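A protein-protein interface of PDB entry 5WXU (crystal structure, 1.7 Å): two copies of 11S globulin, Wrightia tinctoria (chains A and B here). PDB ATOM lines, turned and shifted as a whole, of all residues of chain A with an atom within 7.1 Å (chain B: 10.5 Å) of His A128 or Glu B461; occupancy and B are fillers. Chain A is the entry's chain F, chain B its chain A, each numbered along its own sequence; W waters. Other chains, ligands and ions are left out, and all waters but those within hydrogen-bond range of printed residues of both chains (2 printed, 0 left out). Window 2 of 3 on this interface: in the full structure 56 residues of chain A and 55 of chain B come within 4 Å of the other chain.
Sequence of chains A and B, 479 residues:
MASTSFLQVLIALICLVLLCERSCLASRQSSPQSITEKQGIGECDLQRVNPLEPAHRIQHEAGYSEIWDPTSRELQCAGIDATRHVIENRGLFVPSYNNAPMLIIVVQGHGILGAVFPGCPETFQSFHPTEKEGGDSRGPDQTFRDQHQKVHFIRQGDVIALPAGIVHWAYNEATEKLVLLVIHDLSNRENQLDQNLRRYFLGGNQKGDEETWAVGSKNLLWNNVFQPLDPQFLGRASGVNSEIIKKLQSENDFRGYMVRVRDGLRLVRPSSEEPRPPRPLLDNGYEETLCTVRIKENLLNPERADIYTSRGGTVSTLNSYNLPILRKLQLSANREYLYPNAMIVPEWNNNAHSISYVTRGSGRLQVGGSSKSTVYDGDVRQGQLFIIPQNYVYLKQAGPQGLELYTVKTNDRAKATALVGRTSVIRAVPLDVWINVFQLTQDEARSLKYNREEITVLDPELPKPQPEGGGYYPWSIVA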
ATOM      1  N   GLN A 125      14.173   6.715  -6.915  1.00  0.00           N
ATOM      2  CA  GLN A 125      13.013   7.542  -7.239  1.00  0.00           C
ATOM      3  C   GLN A 125      12.156   6.953  -8.345  1.00  0.00           C
ATOM      4  O   GLN A 125      12.661   6.611  -9.406  1.00  0.00           O
ATOM      5  CB  GLN A 125      13.552   8.868  -7.741  1.00  0.00           C
ATOM      6  CG  GLN A 125      14.521   9.594  -6.804  1.00  0.00           C
ATOM      7  CD  GLN A 125      15.393  10.584  -7.577  1.00  0.00           C
ATOM      8  OE1 GLN A 125      15.035  11.711  -7.727  1.00  0.00           O
ATOM      9  NE2 GLN A 125      16.518  10.131  -8.091  1.00  0.00           N
ATOM     10  N   SER A 126      10.826   6.965  -8.127  1.00  0.00           N
ATOM     11  CA  SER A 126       9.829   6.637  -9.196  1.00  0.00           C
ATOM     12  C   SER A 126       8.692   7.632  -9.096  1.00  0.00           C
ATOM     13  O   SER A 126       8.143   7.850  -8.021  1.00  0.00           O
ATOM     14  CB  SER A 126       9.239   5.260  -8.971  1.00  0.00           C
ATOM     15  OG  SER A 126       8.235   4.973  -9.936  1.00  0.00           O
ATOM     16  N   PHE A 127       8.421   8.268 -10.209  1.00  0.00           N
ATOM     17  CA  PHE A 127       7.362   9.251 -10.334  1.00  0.00           C
ATOM     18  C   PHE A 127       6.108   8.677 -11.023  1.00  0.00           C
ATOM     19  O   PHE A 127       5.171   9.411 -11.316  1.00  0.00           O
ATOM     20  CB  PHE A 127       7.944  10.520 -10.970  1.00  0.00           C
ATOM     21  CG  PHE A 127       9.044  11.099 -10.133  1.00  0.00           C
ATOM     22  CD1 PHE A 127       8.742  11.799  -8.987  1.00  0.00           C
ATOM     23  CD2 PHE A 127      10.421  10.826 -10.430  1.00  0.00           C
ATOM     24  CE1 PHE A 127       9.760  12.229  -8.140  1.00  0.00           C
ATOM     25  CE2 PHE A 127      11.428  11.316  -9.630  1.00  0.00           C
ATOM     26  CZ  PHE A 127      11.105  11.972  -8.460  1.00  0.00           C
ATOM     27  N   HIS A 128       6.067   7.361 -11.169  1.00  0.00           N
ATOM     28  CA  HIS A 128       4.969   6.625 -11.839  1.00  0.00           C
ATOM     29  C   HIS A 128       4.514   5.464 -10.978  1.00  0.00           C
ATOM     30  O   HIS A 128       5.373   4.818 -10.330  1.00  0.00           O
ATOM     31  CB  HIS A 128       5.453   6.038 -13.158  1.00  0.00           C
ATOM     32  CG  HIS A 128       5.783   7.081 -14.181  1.00  0.00           C
ATOM     33  ND1 HIS A 128       7.077   7.360 -14.581  1.00  0.00           N
ATOM     34  CD2 HIS A 128       4.985   7.932 -14.873  1.00  0.00           C
ATOM     35  CE1 HIS A 128       7.059   8.324 -15.489  1.00  0.00           C
ATOM     36  NE2 HIS A 128       5.802   8.687 -15.686  1.00  0.00           N
ATOM     37  N   PRO A 129       3.213   5.139 -10.950  1.00  0.00           N
ATOM     38  CA  PRO A 129       2.092   5.825 -11.659  1.00  0.00           C
ATOM     39  C   PRO A 129       1.637   7.193 -11.107  1.00  0.00           C
ATOM     40  O   PRO A 129       1.965   7.554  -9.987  1.00  0.00           O
ATOM     41  CB  PRO A 129       0.944   4.817 -11.515  1.00  0.00           C
ATOM     42  CG  PRO A 129       1.274   4.020 -10.275  1.00  0.00           C
ATOM     43  CD  PRO A 129       2.766   3.933 -10.214  1.00  0.00           C
ATOM     44  N   THR A 130       0.835   7.901 -11.898  1.00  0.00           N
ATOM     45  CA  THR A 130       0.408   9.286 -11.629  1.00  0.00           C
ATOM     46  C   THR A 130      -1.116   9.373 -11.479  1.00  0.00           C
ATOM     47  O   THR A 130      -1.685   9.029 -10.439  1.00  0.00           O
ATOM     48  CB  THR A 130       0.853  10.191 -12.798  1.00  0.00           C
ATOM     49  OG1 THR A 130       2.208   9.880 -13.142  1.00  0.00           O
ATOM     50  CG2 THR A 130       0.750  11.656 -12.449  1.00  0.00           C
ATOM     51  N   THR A 143       2.110   1.420  -4.918  1.00  0.00           N
ATOM     52  CA  THR A 143       3.125   1.992  -4.067  1.00  0.00           C
ATOM     53  C   THR A 143       4.440   2.035  -4.791  1.00  0.00           C
ATOM     54  O   THR A 143       5.467   2.347  -4.176  1.00  0.00           O
ATOM     55  CB  THR A 143       3.341   1.187  -2.783  1.00  0.00           C
ATOM     56  OG1 THR A 143       4.018  -0.031  -3.086  1.00  0.00           O
ATOM     57  CG2 THR A 143       2.026   0.885  -2.127  1.00  0.00           C
ATOM     58  N   PHE A 144       4.401   1.672  -6.079  1.00  0.00           N
ATOM     59  CA  PHE A 144       5.491   1.976  -7.006  1.00  0.00           C
ATOM     60  C   PHE A 144       5.738   3.466  -7.225  1.00  0.00           C
ATOM     61  O   PHE A 144       6.788   3.769  -7.756  1.00  0.00           O
ATOM     62  CB  PHE A 144       5.331   1.270  -8.381  1.00  0.00           C
ATOM     63  CG  PHE A 144       5.697  -0.196  -8.358  1.00  0.00           C
ATOM     64  CD1 PHE A 144       4.752  -1.180  -8.714  1.00  0.00           C
ATOM     65  CD2 PHE A 144       6.986  -0.607  -7.946  1.00  0.00           C
ATOM     66  CE1 PHE A 144       5.083  -2.531  -8.664  1.00  0.00           C
ATOM     67  CE2 PHE A 144       7.317  -1.957  -7.905  1.00  0.00           C
ATOM     68  CZ  PHE A 144       6.366  -2.925  -8.266  1.00  0.00           C
ATOM     69  N   ARG A 145       4.826   4.395  -6.880  1.00  0.00           N
ATOM     70  CA  ARG A 145       5.223   5.804  -6.905  1.00  0.00           C
ATOM     71  C   ARG A 145       5.799   6.124  -5.515  1.00  0.00           C
ATOM     72  O   ARG A 145       5.042   6.221  -4.548  1.00  0.00           O
ATOM     73  CB  ARG A 145       4.054   6.745  -7.208  1.00  0.00           C
ATOM     74  CG  ARG A 145       4.369   8.235  -7.100  1.00  0.00           C
ATOM     75  CD  ARG A 145       3.221   9.187  -7.545  1.00  0.00           C
ATOM     76  NE  ARG A 145       2.504   9.855  -6.420  1.00  0.00           N
ATOM     77  CZ  ARG A 145       1.378   9.427  -5.804  1.00  0.00           C
ATOM     78  NH1 ARG A 145       0.719   8.317  -6.174  1.00  0.00           N
ATOM     79  NH2 ARG A 145       0.868  10.156  -4.808  1.00  0.00           N
ATOM     80  N   ASP A 146       7.126   6.299  -5.423  1.00  0.00           N
ATOM     81  CA  ASP A 146       7.790   6.454  -4.113  1.00  0.00           C
ATOM     82  C   ASP A 146       9.200   6.994  -4.330  1.00  0.00           C
ATOM     83  O   ASP A 146       9.745   6.922  -5.447  1.00  0.00           O
ATOM     84  CB  ASP A 146       7.857   5.092  -3.417  1.00  0.00           C
ATOM     85  CG  ASP A 146       8.242   5.164  -1.953  1.00  0.00           C
ATOM     86  OD1 ASP A 146       8.220   6.203  -1.281  1.00  0.00           O
ATOM     87  OD2 ASP A 146       8.569   4.128  -1.397  1.00  0.00           O
ATOM     88  N   TYR B 308      18.941   6.396  -8.838  1.00  0.00           N
ATOM     89  CA  TYR B 308      18.130   5.693  -9.828  1.00  0.00           C
ATOM     90  C   TYR B 308      16.813   6.443  -9.984  1.00  0.00           C
ATOM     91  O   TYR B 308      16.152   6.740  -8.983  1.00  0.00           O
ATOM     92  CB  TYR B 308      17.863   4.278  -9.342  1.00  0.00           C
ATOM     93  CG  TYR B 308      16.751   3.595 -10.133  1.00  0.00           C
ATOM     94  CD1 TYR B 308      16.787   3.493 -11.537  1.00  0.00           C
ATOM     95  CD2 TYR B 308      15.626   3.125  -9.462  1.00  0.00           C
ATOM     96  CE1 TYR B 308      15.784   2.867 -12.224  1.00  0.00           C
ATOM     97  CE2 TYR B 308      14.610   2.498 -10.147  1.00  0.00           C
ATOM     98  CZ  TYR B 308      14.693   2.358 -11.513  1.00  0.00           C
ATOM     99  OH  TYR B 308      13.618   1.708 -12.151  1.00  0.00           O
ATOM    100  N   THR B 309      16.475   6.781 -11.225  1.00  0.00           N
ATOM    101  CA  THR B 309      15.144   7.366 -11.570  1.00  0.00           C
ATOM    102  C   THR B 309      14.485   6.393 -12.498  1.00  0.00           C
ATOM    103  O   THR B 309      14.947   6.198 -13.628  1.00  0.00           O
ATOM    104  CB  THR B 309      15.303   8.736 -12.218  1.00  0.00           C
ATOM    105  OG1 THR B 309      15.894   9.637 -11.253  1.00  0.00           O
ATOM    106  CG2 THR B 309      13.906   9.316 -12.550  1.00  0.00           C
ATOM    107  N   SER B 310      13.364   5.805 -12.055  1.00  0.00           N
ATOM    108  CA  SER B 310      12.594   4.919 -12.903  1.00  0.00           C
ATOM    109  C   SER B 310      12.310   5.626 -14.241  1.00  0.00           C
ATOM    110  O   SER B 310      11.969   6.819 -14.254  1.00  0.00           O
ATOM    111  CB  SER B 310      11.273   4.543 -12.198  1.00  0.00           C
ATOM    112  OG  SER B 310      10.725   3.513 -12.942  1.00  0.00           O
ATOM    113  N   ARG B 311      12.504   4.884 -15.333  1.00  0.00           N
ATOM    114  CA  ARG B 311      12.370   5.360 -16.709  1.00  0.00           C
ATOM    115  C   ARG B 311      13.443   6.327 -17.193  1.00  0.00           C
ATOM    116  O   ARG B 311      13.489   6.690 -18.387  1.00  0.00           O
ATOM    117  CB  ARG B 311      10.944   5.933 -16.927  1.00  0.00           C
ATOM    118  CG  ARG B 311       9.927   4.895 -16.662  1.00  0.00           C
ATOM    119  CD  ARG B 311       8.544   5.423 -16.895  1.00  0.00           C
ATOM    120  NE  ARG B 311       7.562   4.412 -16.463  1.00  0.00           N
ATOM    121  CZ  ARG B 311       6.232   4.477 -16.637  1.00  0.00           C
ATOM    122  NH1 ARG B 311       5.654   5.516 -17.254  1.00  0.00           N
ATOM    123  NH2 ARG B 311       5.476   3.489 -16.170  1.00  0.00           N
ATOM    124  N   GLY B 312      14.373   6.692 -16.310  1.00  0.00           N
ATOM    125  CA  GLY B 312      15.405   7.639 -16.657  1.00  0.00           C
ATOM    126  C   GLY B 312      16.784   6.996 -16.673  1.00  0.00           C
ATOM    127  O   GLY B 312      17.494   7.118 -17.652  1.00  0.00           O
ATOM    128  N   GLY B 313      17.142   6.276 -15.641  1.00  0.00           N
ATOM    129  CA  GLY B 313      18.472   5.613 -15.622  1.00  0.00           C
ATOM    130  C   GLY B 313      19.152   5.690 -14.282  1.00  0.00           C
ATOM    131  O   GLY B 313      18.515   5.885 -13.295  1.00  0.00           O
ATOM    132  N   TYR B 339      18.240   5.816 -20.184  1.00  0.00           N
ATOM    133  CA  TYR B 339      17.256   5.289 -21.142  1.00  0.00           C
ATOM    134  C   TYR B 339      17.032   6.261 -22.270  1.00  0.00           C
ATOM    135  O   TYR B 339      17.370   7.428 -22.166  1.00  0.00           O
ATOM    136  CB  TYR B 339      15.943   4.947 -20.445  1.00  0.00           C
ATOM    137  CG  TYR B 339      16.108   3.773 -19.577  1.00  0.00           C
ATOM    138  CD1 TYR B 339      16.270   2.472 -20.113  1.00  0.00           C
ATOM    139  CD2 TYR B 339      16.152   3.918 -18.223  1.00  0.00           C
ATOM    140  CE1 TYR B 339      16.456   1.374 -19.277  1.00  0.00           C
ATOM    141  CE2 TYR B 339      16.351   2.828 -17.371  1.00  0.00           C
ATOM    142  CZ  TYR B 339      16.510   1.563 -17.884  1.00  0.00           C
ATOM    143  OH  TYR B 339      16.688   0.458 -17.028  1.00  0.00           O
ATOM    144  N   PRO B 340      16.397   5.784 -23.378  1.00  0.00           N
ATOM    145  CA  PRO B 340      16.237   6.724 -24.497  1.00  0.00           C
ATOM    146  C   PRO B 340      15.550   8.033 -24.088  1.00  0.00           C
ATOM    147  O   PRO B 340      14.531   7.994 -23.339  1.00  0.00           O
ATOM    148  CB  PRO B 340      15.358   5.938 -25.497  1.00  0.00           C
ATOM    149  CG  PRO B 340      15.710   4.521 -25.198  1.00  0.00           C
ATOM    150  CD  PRO B 340      15.896   4.424 -23.712  1.00  0.00           C
ATOM    151  N   ASN B 341      16.155   9.137 -24.591  1.00  0.00           N
ATOM    152  CA  ASN B 341      15.712  10.524 -24.353  1.00  0.00           C
ATOM    153  C   ASN B 341      15.828  11.031 -22.938  1.00  0.00           C
ATOM    154  O   ASN B 341      15.482  12.180 -22.680  1.00  0.00           O
ATOM    155  CB  ASN B 341      14.264  10.714 -24.850  1.00  0.00           C
ATOM    156  CG  ASN B 341      14.083  10.140 -26.236  1.00  0.00           C
ATOM    157  OD1 ASN B 341      13.256   9.214 -26.451  1.00  0.00           O
ATOM    158  ND2 ASN B 341      14.911  10.580 -27.155  1.00  0.00           N
ATOM    159  N   ALA B 342      16.357  10.229 -22.009  1.00  0.00           N
ATOM    160  CA  ALA B 342      16.538  10.717 -20.622  1.00  0.00           C
ATOM    161  C   ALA B 342      17.755  11.640 -20.560  1.00  0.00           C
ATOM    162  O   ALA B 342      18.597  11.635 -21.418  1.00  0.00           O
ATOM    163  CB  ALA B 342      16.667   9.554 -19.648  1.00  0.00           C
ATOM    164  N   MET B 343      17.856  12.411 -19.483  1.00  0.00           N
ATOM    165  CA  MET B 343      18.925  13.350 -19.327  1.00  0.00           C
ATOM    166  C   MET B 343      19.544  13.216 -17.935  1.00  0.00           C
ATOM    167  O   MET B 343      18.943  12.703 -16.986  1.00  0.00           O
ATOM    168  CB  MET B 343      18.381  14.783 -19.483  1.00  0.00           C
ATOM    169  CG  MET B 343      17.963  15.202 -20.846  1.00  0.00           C
ATOM    170  SD  MET B 343      17.029  16.787 -20.676  1.00  0.00           S
ATOM    171  CE  MET B 343      17.375  17.666 -22.157  1.00  0.00           C
ATOM    172  N   GLN B 397      21.797  14.460 -23.067  1.00  0.00           N
ATOM    173  CA  GLN B 397      20.556  13.766 -23.312  1.00  0.00           C
ATOM    174  C   GLN B 397      20.806  12.499 -24.169  1.00  0.00           C
ATOM    175  O   GLN B 397      21.356  12.610 -25.228  1.00  0.00           O
ATOM    176  CB  GLN B 397      19.563  14.714 -24.014  1.00  0.00           C
ATOM    177  CG  GLN B 397      18.254  14.000 -24.304  1.00  0.00           C
ATOM    178  CD  GLN B 397      17.070  14.861 -24.730  1.00  0.00           C
ATOM    179  OE1 GLN B 397      17.257  15.925 -25.309  1.00  0.00           O
ATOM    180  NE2 GLN B 397      15.842  14.406 -24.442  1.00  0.00           N
ATOM    181  N   ASN B 451       9.557  22.525 -10.794  1.00  0.00           N
ATOM    182  CA  ASN B 451       9.032  21.678 -11.897  1.00  0.00           C
ATOM    183  C   ASN B 451       9.661  20.286 -12.022  1.00  0.00           C
ATOM    184  O   ASN B 451       8.944  19.289 -12.204  1.00  0.00           O
ATOM    185  CB  ASN B 451       9.005  22.423 -13.213  1.00  0.00           C
ATOM    186  CG  ASN B 451       7.792  23.369 -13.304  1.00  0.00           C
ATOM    187  OD1 ASN B 451       7.025  23.507 -12.355  1.00  0.00           O
ATOM    188  ND2 ASN B 451       7.606  23.942 -14.445  1.00  0.00           N
ATOM    189  N   ARG B 452      10.962  20.177 -11.871  1.00  0.00           N
ATOM    190  CA  ARG B 452      11.566  18.823 -11.850  1.00  0.00           C
ATOM    191  C   ARG B 452      11.796  18.397 -10.395  1.00  0.00           C
ATOM    192  O   ARG B 452      12.503  19.090  -9.640  1.00  0.00           O
ATOM    193  CB  ARG B 452      12.931  18.744 -12.569  1.00  0.00           C
ATOM    194  CG  ARG B 452      13.090  19.389 -13.936  1.00  0.00           C
ATOM    195  CD  ARG B 452      12.257  18.808 -15.034  1.00  0.00           C
ATOM    196  NE  ARG B 452      12.302  17.366 -15.188  1.00  0.00           N
ATOM    197  CZ  ARG B 452      12.479  16.713 -16.353  1.00  0.00           C
ATOM    198  NH1 ARG B 452      12.779  17.342 -17.483  1.00  0.00           N
ATOM    199  NH2 ARG B 452      12.432  15.375 -16.368  1.00  0.00           N
ATOM    200  N   GLU B 453      11.220  17.276 -10.026  1.00  0.00           N
ATOM    201  CA  GLU B 453      11.294  16.759  -8.691  1.00  0.00           C
ATOM    202  C   GLU B 453      12.346  15.668  -8.574  1.00  0.00           C
ATOM    203  O   GLU B 453      12.536  15.112  -7.507  1.00  0.00           O
ATOM    204  CB  GLU B 453       9.900  16.274  -8.296  1.00  0.00           C
ATOM    205  CG  GLU B 453       9.024  17.441  -7.818  1.00  0.00           C
ATOM    206  CD  GLU B 453       9.734  18.344  -6.790  1.00  0.00           C
ATOM    207  OE1 GLU B 453      10.394  17.840  -5.854  1.00  0.00           O
ATOM    208  OE2 GLU B 453       9.646  19.579  -6.889  1.00  0.00           O
ATOM    209  N   GLU B 454      13.027  15.370  -9.676  1.00  0.00           N
ATOM    210  CA  GLU B 454      14.152  14.375  -9.663  1.00  0.00           C
ATOM    211  C   GLU B 454      15.397  14.931  -9.047  1.00  0.00           C
ATOM    212  O   GLU B 454      15.585  16.137  -9.007  1.00  0.00           O
ATOM    213  CB  GLU B 454      14.502  13.991 -11.090  1.00  0.00           C
ATOM    214  CG  GLU B 454      13.271  13.388 -11.819  1.00  0.00           C
ATOM    215  CD  GLU B 454      12.615  14.307 -12.847  1.00  0.00           C
ATOM    216  OE1 GLU B 454      12.356  15.465 -12.560  1.00  0.00           O
ATOM    217  OE2 GLU B 454      12.378  13.852 -13.994  1.00  0.00           O
ATOM    218  N   VAL B 457      19.050  12.336 -12.304  1.00  0.00           N
ATOM    219  CA  VAL B 457      18.679  11.610 -13.526  1.00  0.00           C
ATOM    220  C   VAL B 457      17.225  12.042 -13.815  1.00  0.00           C
ATOM    221  O   VAL B 457      16.405  11.883 -12.950  1.00  0.00           O
ATOM    222  CB  VAL B 457      18.743  10.109 -13.290  1.00  0.00           C
ATOM    223  CG1 VAL B 457      18.418   9.374 -14.578  1.00  0.00           C
ATOM    224  CG2 VAL B 457      20.174   9.731 -12.878  1.00  0.00           C
ATOM    225  N   LEU B 458      16.987  12.572 -14.996  1.00  0.00           N
ATOM    226  CA  LEU B 458      15.665  13.121 -15.382  1.00  0.00           C
ATOM    227  C   LEU B 458      14.949  12.083 -16.226  1.00  0.00           C
ATOM    228  O   LEU B 458      15.528  11.512 -17.141  1.00  0.00           O
ATOM    229  CB  LEU B 458      15.800  14.403 -16.121  1.00  0.00           C
ATOM    230  CG  LEU B 458      16.546  15.525 -15.387  1.00  0.00           C
ATOM    231  CD1 LEU B 458      16.660  16.719 -16.292  1.00  0.00           C
ATOM    232  CD2 LEU B 458      15.793  15.898 -14.120  1.00  0.00           C
ATOM    233  N   ASP B 459      13.680  11.876 -15.857  1.00  0.00           N
ATOM    234  CA  ASP B 459      12.691  11.017 -16.515  1.00  0.00           C
ATOM    235  C   ASP B 459      12.384  11.764 -17.835  1.00  0.00           C
ATOM    236  O   ASP B 459      12.225  12.996 -17.844  1.00  0.00           O
ATOM    237  CB  ASP B 459      11.532  10.939 -15.499  1.00  0.00           C
ATOM    238  CG  ASP B 459      10.471   9.941 -15.813  1.00  0.00           C
ATOM    239  OD1 ASP B 459      10.123   9.728 -16.979  1.00  0.00           O
ATOM    240  OD2 ASP B 459       9.902   9.439 -14.820  1.00  0.00           O
ATOM    241  N   PRO B 460      12.385  11.059 -18.965  1.00  0.00           N
ATOM    242  CA  PRO B 460      12.047  11.727 -20.212  1.00  0.00           C
ATOM    243  C   PRO B 460      10.552  12.046 -20.256  1.00  0.00           C
ATOM    244  O   PRO B 460      10.191  12.976 -20.934  1.00  0.00           O
ATOM    245  CB  PRO B 460      12.427  10.703 -21.285  1.00  0.00           C
ATOM    246  CG  PRO B 460      12.711   9.426 -20.598  1.00  0.00           C
ATOM    247  CD  PRO B 460      12.691   9.633 -19.138  1.00  0.00           C
ATOM    248  N   GLU B 461       9.737  11.256 -19.541  1.00  0.00           N
ATOM    249  CA  GLU B 461       8.313  11.518 -19.291  1.00  0.00           C
ATOM    250  C   GLU B 461       8.030  11.902 -17.803  1.00  0.00           C
ATOM    251  O   GLU B 461       8.341  13.012 -17.340  1.00  0.00           O
ATOM    252  CB  GLU B 461       7.485  10.276 -19.679  1.00  0.00           C
ATOM    253  CG  GLU B 461       6.121  10.621 -20.276  1.00  0.00           C
ATOM    254  CD  GLU B 461       5.311  11.586 -19.407  1.00  0.00           C
ATOM    255  OE1 GLU B 461       5.188  11.333 -18.189  1.00  0.00           O
ATOM    256  OE2 GLU B 461       4.812  12.605 -19.937  1.00  0.00           O
HETATM  257  O   HOH W   1       9.957   8.094 -12.605  1.00  0.00           O
HETATM  258  O   HOH W   2       8.054   4.177 -13.209  1.00  0.00           O
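The backbone carbonyl oxygen (O) of Tyr B308 lies within hydrogen-bond range of the backbone NH (N) of Gln A125.
The side-chain hydroxyl of Thr B309 sits at hydrogen-bond distance from the side-chain amide nitrogen of Gln A125, at 3.3 Å.
The backbone NH (N) of Ser B310 sits at hydrogen-bond distance from the backbone carbonyl oxygen (O) of Gln A125, at 2.9 Å.
The side-chain hydroxyl (OG1) of Thr B309 sits at hydrogen-bond distance from the backbone carbonyl oxygen (O) of Val B457, at 2.9 Å.
O of Asp B459 sits at hydrogen-bond distance from NH2 of Arg B452 (2.8 Å).
The side-chain carboxylate (OE2) of Glu B454 lies within hydrogen-bond range of the backbone NH (N) of Asp B459 (3.0 Å).
The side-chain hydroxyl (OG) of Ser A126 sits at hydrogen-bond distance from the backbone carbonyl oxygen (O) of His A128, at 2.9 Å.
The side-chain hydroxyl (OG) of Ser A126 is in hydrogen-bond range of the backbone carbonyl oxygen (O) of Phe A144.
O of Asp A146 lies within hydrogen-bond range of N of Ser A126 (2.9 Å).
Gln A125 touches Glu B454.
Ser B310 touches Ser A126.
CZ of Phe A127 touches O of Glu B453 (3.6 Å).
Phe A127 touches Glu B454.
ND1 of His A128 touches CD of Arg B311, 3.4 Å away.
OD2 of Asp B459 touches CE1 of His A128, at 3.1 Å.
Glu B461 touches His A128.
Of chain B, only Arg B311, Asp B459 and Glu B461 come within 4 Å of His A128.
No residue of chain B comes within 4 Å of Pro A129.
Arg A145 touches none of the printed residues of chain B.
Printed residues of chain A within 4 Å of Thr B309: Gln A125 (3.3 Å).
Pro B340 touches none of the printed residues of chain A.
Of the printed residues of chain A, Glu B454 touches Gln A125 and Phe A127.
Of the printed residues of chain A, Asp B459 touches His A128 (3.1 Å).
The nearest residue of chain B that does not touch His A128 is Ser B310 (4.9 Å).
The nearest residue of chain A that does not touch Glu B461 is Thr A130 (6.0 Å).
Of the 10 printed residues of chain A, 4 touch a printed residue of chain B.
Of the 21 printed residues of chain B, 8 touch a printed residue of chain A.
No position is printed for both chains.
Of the 10 pairs that touch across the chains among the printed residues, none has its exchanged pair printed and touching as well.
Water W1 lies within hydrogen-bond range of OD2 of Asp B459 (2.6 Å), N of Phe A127 (2.9 Å) and O of Ser B310 (2.9 Å).
Water W2 lies within hydrogen-bond range of OG of Ser B310 (2.8 Å), NE of Arg B311 (3.3 Å) and OG of Ser A126 (3.4 Å).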
